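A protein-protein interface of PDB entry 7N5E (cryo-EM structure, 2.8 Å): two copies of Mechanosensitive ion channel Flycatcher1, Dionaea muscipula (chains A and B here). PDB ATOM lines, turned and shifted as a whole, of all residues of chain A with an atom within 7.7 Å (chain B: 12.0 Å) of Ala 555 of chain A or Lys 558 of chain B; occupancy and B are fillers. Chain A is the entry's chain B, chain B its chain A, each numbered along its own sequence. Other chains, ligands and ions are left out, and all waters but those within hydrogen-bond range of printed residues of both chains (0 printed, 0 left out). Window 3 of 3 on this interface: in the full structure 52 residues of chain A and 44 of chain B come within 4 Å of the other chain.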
ATOM      1  N   VAL A 546     -21.500  -5.206  -1.428  1.00  0.00           N
ATOM      2  CA  VAL A 546     -21.569  -5.848  -0.152  1.00  0.00           C
ATOM      3  C   VAL A 546     -20.215  -6.392   0.224  1.00  0.00           C
ATOM      4  O   VAL A 546     -19.812  -6.252   1.369  1.00  0.00           O
ATOM      5  CB  VAL A 546     -22.614  -6.932  -0.130  1.00  0.00           C
ATOM      6  CG1 VAL A 546     -22.535  -7.715   1.191  1.00  0.00           C
ATOM      7  CG2 VAL A 546     -23.947  -6.287  -0.290  1.00  0.00           C
ATOM      8  N   TRP A 548     -17.296  -5.250  -0.533  1.00  0.00           N
ATOM      9  CA  TRP A 548     -16.464  -4.147  -0.097  1.00  0.00           C
ATOM     10  C   TRP A 548     -16.784  -3.748   1.314  1.00  0.00           C
ATOM     11  O   TRP A 548     -15.902  -3.633   2.162  1.00  0.00           O
ATOM     12  CB  TRP A 548     -16.682  -2.949  -0.973  1.00  0.00           C
ATOM     13  CG  TRP A 548     -15.896  -1.859  -0.593  1.00  0.00           C
ATOM     14  CD1 TRP A 548     -14.602  -1.684  -0.842  1.00  0.00           C
ATOM     15  CD2 TRP A 548     -16.331  -0.705   0.065  1.00  0.00           C
ATOM     16  NE1 TRP A 548     -14.198  -0.503  -0.352  1.00  0.00           N
ATOM     17  CE2 TRP A 548     -15.241   0.112   0.194  1.00  0.00           C
ATOM     18  CE3 TRP A 548     -17.546  -0.289   0.542  1.00  0.00           C
ATOM     19  CZ2 TRP A 548     -15.318   1.317   0.785  1.00  0.00           C
ATOM     20  CZ3 TRP A 548     -17.628   0.937   1.140  1.00  0.00           C
ATOM     21  CH2 TRP A 548     -16.538   1.720   1.260  1.00  0.00           C
ATOM     22  N   LEU A 549     -18.058  -3.628   1.620  1.00  0.00           N
ATOM     23  CA  LEU A 549     -18.448  -3.222   2.944  1.00  0.00           C
ATOM     24  C   LEU A 549     -17.988  -4.184   4.016  1.00  0.00           C
ATOM     25  O   LEU A 549     -17.688  -3.791   5.151  1.00  0.00           O
ATOM     26  CB  LEU A 549     -19.956  -3.123   3.016  1.00  0.00           C
ATOM     27  CG  LEU A 549     -20.607  -2.003   2.270  1.00  0.00           C
ATOM     28  CD1 LEU A 549     -22.104  -2.223   2.274  1.00  0.00           C
ATOM     29  CD2 LEU A 549     -20.295  -0.699   2.934  1.00  0.00           C
ATOM     30  N   ILE A 550     -17.942  -5.448   3.692  1.00  0.00           N
ATOM     31  CA  ILE A 550     -17.531  -6.417   4.663  1.00  0.00           C
ATOM     32  C   ILE A 550     -16.017  -6.599   4.755  1.00  0.00           C
ATOM     33  O   ILE A 550     -15.463  -6.574   5.850  1.00  0.00           O
ATOM     34  CB  ILE A 550     -18.192  -7.736   4.320  1.00  0.00           C
ATOM     35  CG1 ILE A 550     -19.704  -7.546   4.295  1.00  0.00           C
ATOM     36  CG2 ILE A 550     -17.780  -8.840   5.273  1.00  0.00           C
ATOM     37  CD1 ILE A 550     -20.352  -7.072   5.530  1.00  0.00           C
ATOM     38  N   VAL A 551     -15.328  -6.756   3.641  1.00  0.00           N
ATOM     39  CA  VAL A 551     -13.900  -7.040   3.675  1.00  0.00           C
ATOM     40  C   VAL A 551     -13.066  -5.888   4.192  1.00  0.00           C
ATOM     41  O   VAL A 551     -12.032  -6.119   4.808  1.00  0.00           O
ATOM     42  CB  VAL A 551     -13.376  -7.498   2.311  1.00  0.00           C
ATOM     43  CG1 VAL A 551     -13.278  -6.364   1.341  1.00  0.00           C
ATOM     44  CG2 VAL A 551     -12.015  -8.137   2.482  1.00  0.00           C
ATOM     45  N   THR A 552     -13.488  -4.646   3.985  1.00  0.00           N
ATOM     46  CA  THR A 552     -12.686  -3.552   4.504  1.00  0.00           C
ATOM     47  C   THR A 552     -12.992  -3.324   5.975  1.00  0.00           C
ATOM     48  O   THR A 552     -12.347  -2.499   6.623  1.00  0.00           O
ATOM     49  CB  THR A 552     -12.945  -2.215   3.807  1.00  0.00           C
ATOM     50  OG1 THR A 552     -14.278  -1.809   4.073  1.00  0.00           O
ATOM     51  CG2 THR A 552     -12.749  -2.329   2.316  1.00  0.00           C
ATOM     52  N   GLY A 553     -14.036  -3.963   6.491  1.00  0.00           N
ATOM     53  CA  GLY A 553     -14.432  -3.802   7.866  1.00  0.00           C
ATOM     54  C   GLY A 553     -15.235  -2.549   8.110  1.00  0.00           C
ATOM     55  O   GLY A 553     -15.547  -2.233   9.254  1.00  0.00           O
ATOM     56  N   ILE A 554     -15.578  -1.825   7.061  1.00  0.00           N
ATOM     57  CA  ILE A 554     -16.305  -0.590   7.252  1.00  0.00           C
ATOM     58  C   ILE A 554     -17.696  -0.798   7.812  1.00  0.00           C
ATOM     59  O   ILE A 554     -18.188   0.038   8.565  1.00  0.00           O
ATOM     60  CB  ILE A 554     -16.317   0.225   5.951  1.00  0.00           C
ATOM     61  CG1 ILE A 554     -16.788   1.656   6.227  1.00  0.00           C
ATOM     62  CG2 ILE A 554     -17.122  -0.447   4.897  1.00  0.00           C
ATOM     63  CD1 ILE A 554     -16.549   2.633   5.070  1.00  0.00           C
ATOM     64  N   ALA A 555     -18.353  -1.875   7.438  1.00  0.00           N
ATOM     65  CA  ALA A 555     -19.658  -2.133   7.988  1.00  0.00           C
ATOM     66  C   ALA A 555     -19.545  -2.741   9.369  1.00  0.00           C
ATOM     67  O   ALA A 555     -18.662  -3.557   9.643  1.00  0.00           O
ATOM     68  CB  ALA A 555     -20.442  -3.044   7.077  1.00  0.00           C
ATOM     69  N   THR A 556     -20.507  -2.427  10.207  1.00  0.00           N
ATOM     70  CA  THR A 556     -20.583  -3.026  11.513  1.00  0.00           C
ATOM     71  C   THR A 556     -21.628  -4.084  11.514  1.00  0.00           C
ATOM     72  O   THR A 556     -22.426  -4.159  10.581  1.00  0.00           O
ATOM     73  CB  THR A 556     -20.912  -1.995  12.579  1.00  0.00           C
ATOM     74  OG1 THR A 556     -20.844  -2.621  13.868  1.00  0.00           O
ATOM     75  CG2 THR A 556     -22.318  -1.423  12.350  1.00  0.00           C
ATOM     76  N   THR A 557     -21.699  -4.840  12.581  1.00  0.00           N
ATOM     77  CA  THR A 557     -22.616  -5.939  12.609  1.00  0.00           C
ATOM     78  C   THR A 557     -24.051  -5.652  12.879  1.00  0.00           C
ATOM     79  O   THR A 557     -24.912  -6.434  12.489  1.00  0.00           O
ATOM     80  CB  THR A 557     -22.144  -6.987  13.594  1.00  0.00           C
ATOM     81  OG1 THR A 557     -22.021  -6.393  14.882  1.00  0.00           O
ATOM     82  CG2 THR A 557     -20.831  -7.524  13.143  1.00  0.00           C
ATOM     83  N   LYS A 558     -24.377  -4.531  13.480  1.00  0.00           N
ATOM     84  CA  LYS A 558     -25.790  -4.313  13.675  1.00  0.00           C
ATOM     85  C   LYS A 558     -26.459  -3.971  12.357  1.00  0.00           C
ATOM     86  O   LYS A 558     -27.624  -4.306  12.121  1.00  0.00           O
ATOM     87  CB  LYS A 558     -26.069  -3.184  14.640  1.00  0.00           C
ATOM     88  CG  LYS A 558     -27.562  -2.949  14.923  1.00  0.00           C
ATOM     89  CD  LYS A 558     -28.191  -4.105  15.705  1.00  0.00           C
ATOM     90  CE  LYS A 558     -29.674  -3.863  15.982  1.00  0.00           C
ATOM     91  NZ  LYS A 558     -29.876  -2.687  16.884  1.00  0.00           N
ATOM     92  N   LEU A 559     -25.711  -3.298  11.490  1.00  0.00           N
ATOM     93  CA  LEU A 559     -26.261  -2.882  10.230  1.00  0.00           C
ATOM     94  C   LEU A 559     -26.262  -4.068   9.312  1.00  0.00           C
ATOM     95  O   LEU A 559     -27.172  -4.194   8.505  1.00  0.00           O
ATOM     96  CB  LEU A 559     -25.531  -1.722   9.595  1.00  0.00           C
ATOM     97  CG  LEU A 559     -25.596  -0.372  10.367  1.00  0.00           C
ATOM     98  CD1 LEU A 559     -24.740   0.642   9.629  1.00  0.00           C
ATOM     99  CD2 LEU A 559     -27.044   0.126  10.501  1.00  0.00           C
ATOM    100  N   ILE A 560     -25.289  -4.957   9.441  1.00  0.00           N
ATOM    101  CA  ILE A 560     -25.281  -6.142   8.611  1.00  0.00           C
ATOM    102  C   ILE A 560     -26.483  -6.963   8.958  1.00  0.00           C
ATOM    103  O   ILE A 560     -27.148  -7.489   8.070  1.00  0.00           O
ATOM    104  CB  ILE A 560     -24.007  -6.930   8.775  1.00  0.00           C
ATOM    105  CG1 ILE A 560     -22.909  -6.094   8.194  1.00  0.00           C
ATOM    106  CG2 ILE A 560     -24.121  -8.311   8.075  1.00  0.00           C
ATOM    107  CD1 ILE A 560     -21.551  -6.528   8.576  1.00  0.00           C
ATOM    108  N   VAL A 561     -26.778  -7.099  10.234  1.00  0.00           N
ATOM    109  CA  VAL A 561     -27.946  -7.849  10.577  1.00  0.00           C
ATOM    110  C   VAL A 561     -29.213  -7.191  10.076  1.00  0.00           C
ATOM    111  O   VAL A 561     -30.076  -7.891   9.546  1.00  0.00           O
ATOM    112  CB  VAL A 561     -28.018  -8.087  12.061  1.00  0.00           C
ATOM    113  CG1 VAL A 561     -29.364  -8.705  12.433  1.00  0.00           C
ATOM    114  CG2 VAL A 561     -26.890  -9.025  12.430  1.00  0.00           C
ATOM    115  N   LEU A 563     -29.567  -5.316   7.479  1.00  0.00           N
ATOM    116  CA  LEU A 563     -29.534  -5.460   6.040  1.00  0.00           C
ATOM    117  C   LEU A 563     -30.011  -6.826   5.616  1.00  0.00           C
ATOM    118  O   LEU A 563     -30.847  -6.943   4.713  1.00  0.00           O
ATOM    119  CB  LEU A 563     -28.099  -5.288   5.558  1.00  0.00           C
ATOM    120  CG  LEU A 563     -27.810  -5.482   4.085  1.00  0.00           C
ATOM    121  CD1 LEU A 563     -28.563  -4.460   3.269  1.00  0.00           C
ATOM    122  CD2 LEU A 563     -26.289  -5.383   3.873  1.00  0.00           C
ATOM    123  N   SER A 564     -29.512  -7.872   6.270  1.00  0.00           N
ATOM    124  CA  SER A 564     -29.940  -9.206   5.927  1.00  0.00           C
ATOM    125  C   SER A 564     -31.384  -9.435   6.283  1.00  0.00           C
ATOM    126  O   SER A 564     -32.105 -10.107   5.542  1.00  0.00           O
ATOM    127  CB  SER A 564     -29.083 -10.241   6.592  1.00  0.00           C
ATOM    128  OG  SER A 564     -27.801 -10.245   6.046  1.00  0.00           O
ATOM    129  N   VAL B 546     -18.858 -24.062   1.642  1.00  0.00           N
ATOM    130  CA  VAL B 546     -19.442 -23.436   2.795  1.00  0.00           C
ATOM    131  C   VAL B 546     -19.129 -24.199   4.046  1.00  0.00           C
ATOM    132  O   VAL B 546     -18.801 -23.590   5.058  1.00  0.00           O
ATOM    133  CB  VAL B 546     -20.936 -23.279   2.653  1.00  0.00           C
ATOM    134  CG1 VAL B 546     -21.537 -22.776   3.988  1.00  0.00           C
ATOM    135  CG2 VAL B 546     -21.204 -22.301   1.531  1.00  0.00           C
ATOM    136  N   LEU B 549     -15.677 -23.383   5.274  1.00  0.00           N
ATOM    137  CA  LEU B 549     -15.537 -22.072   5.861  1.00  0.00           C
ATOM    138  C   LEU B 549     -16.116 -21.969   7.236  1.00  0.00           C
ATOM    139  O   LEU B 549     -15.620 -21.209   8.069  1.00  0.00           O
ATOM    140  CB  LEU B 549     -16.268 -21.049   5.010  1.00  0.00           C
ATOM    141  CG  LEU B 549     -15.695 -20.732   3.669  1.00  0.00           C
ATOM    142  CD1 LEU B 549     -16.701 -19.892   2.902  1.00  0.00           C
ATOM    143  CD2 LEU B 549     -14.387 -19.966   3.840  1.00  0.00           C
ATOM    144  N   ILE B 550     -17.185 -22.676   7.502  1.00  0.00           N
ATOM    145  CA  ILE B 550     -17.752 -22.495   8.804  1.00  0.00           C
ATOM    146  C   ILE B 550     -17.154 -23.425   9.859  1.00  0.00           C
ATOM    147  O   ILE B 550     -16.892 -22.985  10.975  1.00  0.00           O
ATOM    148  CB  ILE B 550     -19.280 -22.556   8.707  1.00  0.00           C
ATOM    149  CG1 ILE B 550     -19.779 -23.949   8.324  1.00  0.00           C
ATOM    150  CG2 ILE B 550     -19.686 -21.537   7.611  1.00  0.00           C
ATOM    151  CD1 ILE B 550     -21.264 -24.129   8.346  1.00  0.00           C
ATOM    152  N   GLY B 553     -13.841 -22.226  11.307  1.00  0.00           N
ATOM    153  CA  GLY B 553     -13.816 -20.971  12.022  1.00  0.00           C
ATOM    154  C   GLY B 553     -13.400 -19.798  11.161  1.00  0.00           C
ATOM    155  O   GLY B 553     -13.282 -18.682  11.657  1.00  0.00           O
ATOM    156  N   ILE B 554     -13.178 -20.024   9.880  1.00  0.00           N
ATOM    157  CA  ILE B 554     -12.780 -18.919   9.045  1.00  0.00           C
ATOM    158  C   ILE B 554     -13.885 -17.915   8.917  1.00  0.00           C
ATOM    159  O   ILE B 554     -13.653 -16.710   9.008  1.00  0.00           O
ATOM    160  CB  ILE B 554     -12.385 -19.392   7.661  1.00  0.00           C
ATOM    161  CG1 ILE B 554     -11.125 -20.184   7.776  1.00  0.00           C
ATOM    162  CG2 ILE B 554     -12.230 -18.197   6.711  1.00  0.00           C
ATOM    163  CD1 ILE B 554     -10.790 -20.967   6.555  1.00  0.00           C
ATOM    164  N   ALA B 555     -15.089 -18.381   8.642  1.00  0.00           N
ATOM    165  CA  ALA B 555     -16.172 -17.443   8.528  1.00  0.00           C
ATOM    166  C   ALA B 555     -16.467 -16.882   9.888  1.00  0.00           C
ATOM    167  O   ALA B 555     -16.597 -17.626  10.857  1.00  0.00           O
ATOM    168  CB  ALA B 555     -17.403 -18.099   7.950  1.00  0.00           C
ATOM    169  N   THR B 556     -16.680 -15.591   9.942  1.00  0.00           N
ATOM    170  CA  THR B 556     -17.025 -14.907  11.167  1.00  0.00           C
ATOM    171  C   THR B 556     -18.493 -14.641  11.272  1.00  0.00           C
ATOM    172  O   THR B 556     -19.247 -14.913  10.342  1.00  0.00           O
ATOM    173  CB  THR B 556     -16.254 -13.610  11.303  1.00  0.00           C
ATOM    174  OG1 THR B 556     -16.496 -13.060  12.607  1.00  0.00           O
ATOM    175  CG2 THR B 556     -16.673 -12.644  10.236  1.00  0.00           C
ATOM    176  N   THR B 557     -18.926 -14.038  12.361  1.00  0.00           N
ATOM    177  CA  THR B 557     -20.352 -13.847  12.551  1.00  0.00           C
ATOM    178  C   THR B 557     -21.004 -13.101  11.423  1.00  0.00           C
ATOM    179  O   THR B 557     -22.059 -13.512  10.953  1.00  0.00           O
ATOM    180  CB  THR B 557     -20.640 -13.110  13.854  1.00  0.00           C
ATOM    181  OG1 THR B 557     -20.156 -13.892  14.952  1.00  0.00           O
ATOM    182  CG2 THR B 557     -22.145 -12.907  14.004  1.00  0.00           C
ATOM    183  N   LYS B 558     -20.408 -12.018  10.960  1.00  0.00           N
ATOM    184  CA  LYS B 558     -21.040 -11.297   9.873  1.00  0.00           C
ATOM    185  C   LYS B 558     -21.087 -12.094   8.580  1.00  0.00           C
ATOM    186  O   LYS B 558     -22.035 -11.956   7.805  1.00  0.00           O
ATOM    187  CB  LYS B 558     -20.378  -9.951   9.663  1.00  0.00           C
ATOM    188  CG  LYS B 558     -18.915  -9.978   9.344  1.00  0.00           C
ATOM    189  CD  LYS B 558     -18.349  -8.610   9.015  1.00  0.00           C
ATOM    190  CE  LYS B 558     -18.294  -7.661  10.196  1.00  0.00           C
ATOM    191  NZ  LYS B 558     -17.419  -6.489   9.892  1.00  0.00           N
ATOM    192  N   LEU B 559     -20.121 -12.961   8.348  1.00  0.00           N
ATOM    193  CA  LEU B 559     -20.152 -13.734   7.135  1.00  0.00           C
ATOM    194  C   LEU B 559     -21.199 -14.791   7.226  1.00  0.00           C
ATOM    195  O   LEU B 559     -21.857 -15.079   6.235  1.00  0.00           O
ATOM    196  CB  LEU B 559     -18.799 -14.339   6.847  1.00  0.00           C
ATOM    197  CG  LEU B 559     -17.683 -13.323   6.476  1.00  0.00           C
ATOM    198  CD1 LEU B 559     -16.351 -14.043   6.395  1.00  0.00           C
ATOM    199  CD2 LEU B 559     -17.987 -12.666   5.131  1.00  0.00           C
ATOM    200  N   ILE B 560     -21.416 -15.328   8.406  1.00  0.00           N
ATOM    201  CA  ILE B 560     -22.436 -16.328   8.565  1.00  0.00           C
ATOM    202  C   ILE B 560     -23.777 -15.706   8.310  1.00  0.00           C
ATOM    203  O   ILE B 560     -24.619 -16.313   7.655  1.00  0.00           O
ATOM    204  CB  ILE B 560     -22.455 -16.938   9.956  1.00  0.00           C
ATOM    205  CG1 ILE B 560     -21.144 -17.690  10.254  1.00  0.00           C
ATOM    206  CG2 ILE B 560     -23.679 -17.837  10.118  1.00  0.00           C
ATOM    207  CD1 ILE B 560     -20.783 -18.808   9.351  1.00  0.00           C
ATOM    208  N   VAL B 561     -23.992 -14.504   8.814  1.00  0.00           N
ATOM    209  CA  VAL B 561     -25.258 -13.838   8.609  1.00  0.00           C
ATOM    210  C   VAL B 561     -25.515 -13.604   7.140  1.00  0.00           C
ATOM    211  O   VAL B 561     -26.629 -13.846   6.667  1.00  0.00           O
ATOM    212  CB  VAL B 561     -25.277 -12.498   9.363  1.00  0.00           C
ATOM    213  CG1 VAL B 561     -26.499 -11.648   8.985  1.00  0.00           C
ATOM    214  CG2 VAL B 561     -25.308 -12.775  10.846  1.00  0.00           C
ATOM    215  N   LEU B 562     -24.520 -13.145   6.404  1.00  0.00           N
ATOM    216  CA  LEU B 562     -24.735 -12.932   4.996  1.00  0.00           C
ATOM    217  C   LEU B 562     -24.926 -14.224   4.230  1.00  0.00           C
ATOM    218  O   LEU B 562     -25.786 -14.280   3.357  1.00  0.00           O
ATOM    219  CB  LEU B 562     -23.582 -12.142   4.446  1.00  0.00           C
ATOM    220  CG  LEU B 562     -23.519 -10.690   4.950  1.00  0.00           C
ATOM    221  CD1 LEU B 562     -22.215 -10.108   4.585  1.00  0.00           C
ATOM    222  CD2 LEU B 562     -24.643  -9.830   4.320  1.00  0.00           C
ATOM    223  N   LEU B 563     -24.190 -15.281   4.560  1.00  0.00           N
ATOM    224  CA  LEU B 563     -24.376 -16.525   3.846  1.00  0.00           C
ATOM    225  C   LEU B 563     -25.736 -17.076   4.115  1.00  0.00           C
ATOM    226  O   LEU B 563     -26.365 -17.627   3.212  1.00  0.00           O
ATOM    227  CB  LEU B 563     -23.371 -17.578   4.290  1.00  0.00           C
ATOM    228  CG  LEU B 563     -21.928 -17.388   3.903  1.00  0.00           C
ATOM    229  CD1 LEU B 563     -21.076 -18.420   4.668  1.00  0.00           C
ATOM    230  CD2 LEU B 563     -21.764 -17.584   2.408  1.00  0.00           C
ATOM    231  N   SER B 564     -26.202 -16.938   5.349  1.00  0.00           N
ATOM    232  CA  SER B 564     -27.491 -17.448   5.723  1.00  0.00           C
ATOM    233  C   SER B 564     -28.561 -16.766   4.927  1.00  0.00           C
ATOM    234  O   SER B 564     -29.447 -17.422   4.372  1.00  0.00           O
ATOM    235  CB  SER B 564     -27.717 -17.231   7.188  1.00  0.00           C
ATOM    236  OG  SER B 564     -28.966 -17.709   7.577  1.00  0.00           O
ATOM    237  N   SER B 565     -28.463 -15.455   4.802  1.00  0.00           N
ATOM    238  CA  SER B 565     -29.433 -14.725   4.031  1.00  0.00           C
ATOM    239  C   SER B 565     -29.391 -15.159   2.579  1.00  0.00           C
ATOM    240  O   SER B 565     -30.420 -15.433   1.968  1.00  0.00           O
ATOM    241  CB  SER B 565     -29.148 -13.258   4.129  1.00  0.00           C
ATOM    242  OG  SER B 565     -30.085 -12.513   3.418  1.00  0.00           O
ATOM    243  N   GLN B 566     -28.199 -15.320   2.016  1.00  0.00           N
ATOM    244  CA  GLN B 566     -28.115 -15.686   0.618  1.00  0.00           C
ATOM    245  C   GLN B 566     -28.774 -17.015   0.356  1.00  0.00           C
ATOM    246  O   GLN B 566     -29.463 -17.171  -0.653  1.00  0.00           O
ATOM    247  CB  GLN B 566     -26.669 -15.749   0.195  1.00  0.00           C
ATOM    248  CG  GLN B 566     -25.998 -14.407   0.125  1.00  0.00           C
ATOM    249  CD  GLN B 566     -24.500 -14.535  -0.053  1.00  0.00           C
ATOM    250  OE1 GLN B 566     -23.953 -15.629   0.123  1.00  0.00           O
ATOM    251  NE2 GLN B 566     -23.833 -13.440  -0.394  1.00  0.00           N
ATOM    252  N   LEU B 567     -28.620 -17.960   1.262  1.00  0.00           N
ATOM    253  CA  LEU B 567     -29.258 -19.230   1.074  1.00  0.00           C
ATOM    254  C   LEU B 567     -30.757 -19.101   1.136  1.00  0.00           C
ATOM    255  O   LEU B 567     -31.456 -19.699   0.322  1.00  0.00           O
ATOM    256  CB  LEU B 567     -28.786 -20.218   2.115  1.00  0.00           C
ATOM    257  CG  LEU B 567     -29.393 -21.628   2.062  1.00  0.00           C
ATOM    258  CD1 LEU B 567     -29.129 -22.290   0.724  1.00  0.00           C
ATOM    259  CD2 LEU B 567     -28.773 -22.452   3.179  1.00  0.00           C
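NZ of Lys 558 of chain B lies within hydrogen-bond range of O of Ala 555 of chain A, at 3.2 Å.
The backbone carbonyl oxygen of Leu 549 of chain A sits at hydrogen-bond distance from the backbone NH of Ala 555 of chain A (3.1 Å).
OG of Ser 564 of chain A lies within hydrogen-bond range of O of Ile 560 of chain A (3.5 Å).
Lys 558 of chain B touches Ile 550 of chain A.
CG2 of Ile 550 of chain A touches CD2 of Leu 559 of chain B, at 3.8 Å.
Leu 562 of chain B touches Ile 550 of chain A (CD1 to CG1, 3.6 Å).
CG2 of Thr 557 of chain A touches CE of Lys 558 of chain B, 3.9 Å away.
Ile 560 of chain A touches Lys 558 of chain B (CD1 to CB, 3.8 Å).
Ile 560 of chain A touches Leu 562 of chain B.
Val 561 of chain B touches Ser 564 of chain A.
Ser 564 of chain A touches Leu 562 of chain B.
Ser 564 of chain A touches Ser 565 of chain B.
Leu 549 of chain A touches none of the printed residues of chain B.
Ile 550 of chain A touches just these residues of chain B: Lys 558 (3.8 Å), Leu 559 (3.8 Å) and Leu 562 (3.6 Å).
No residue of chain B comes within 4 Å of Thr 552 of chain A.
No residue of chain B comes within 4 Å of Gly 553 of chain A.
No residue of chain B comes within 4 Å of Ile 554 of chain A.
Of chain B, only Lys 558 comes within 4 Å of Ala 555 of chain A.
No residue of chain B comes within 4 Å of Thr 556 of chain A.
Of the printed residues of chain B, Thr 557 of chain A touches Lys 558.
Lys 558 of chain A touches none of the printed residues of chain B.
Ile 560 of chain A touches just these residues of chain B: Lys 558 and Leu 562.
Thr 557 of chain B touches none of the printed residues of chain A.
Of chain A, only Ile 550, Ala 555, Thr 557 and Ile 560 come within 4 Å of Lys 558 of chain B.
Printed residues of chain A within 4 Å of Val 561 of chain B: Ser 564 (3.5 Å).
Of the printed residues of chain A, Leu 562 of chain B touches Ile 550 (3.6 Å), Ile 560 (3.97 Å) and Ser 564 (3.6 Å).
Of the printed residues of chain A, Ser 565 of chain B touches Ser 564 (3.8 Å).
The nearest residue of chain B that does not touch Ala 555 of chain A is Leu 562 of chain B (7.7 Å).
The nearest residue of chain A that does not touch Lys 558 of chain B is Gly 553 of chain A (4.5 Å).
Of the 18 printed residues of chain B, 5 touch a printed residue of chain A.
Hydrophobic or aromatic side chains of chain B that line the printed part of chain A: Leu 559, Val 561 and Leu 562.
Of the 17 printed residues of chain A, 5 touch a printed residue of chain B.
Hydrophobic or aromatic side chains of chain A that line the printed part of chain B: Ile 550 and Ile 560.
Among the printed residues, no Asp or Glu carboxylate lies within 4 Å of a Lys or Arg side-chain nitrogen of the other chain.
Ile 550 of chain A touches Lys 558 of chain B, but with the chains exchanged Lys 558 of chain A does not touch Ile 550 of chain B (18.6 Å).
Ile 550 of chain A touches Leu 559 of chain B, but with the chains exchanged Leu 559 of chain A does not touch Ile 550 of chain B (18.7 Å).
Thr 557 of chain A touches Lys 558 of chain B, but with the chains exchanged Lys 558 of chain A does not touch Thr 557 of chain B (8.7 Å).
Ser 564 of chain A touches Val 561 of chain B, but with the chains exchanged Val 561 of chain A does not touch Ser 564 of chain B (9.8 Å).
Positions printed for both chains: 546, 549, 550, 553, 554, 555, 556, 557, 558, 559, 560, 561, 563 and 564.
Of the 10 pairs that touch across the chains among the printed residues, none has its exchanged pair printed and touching as well.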
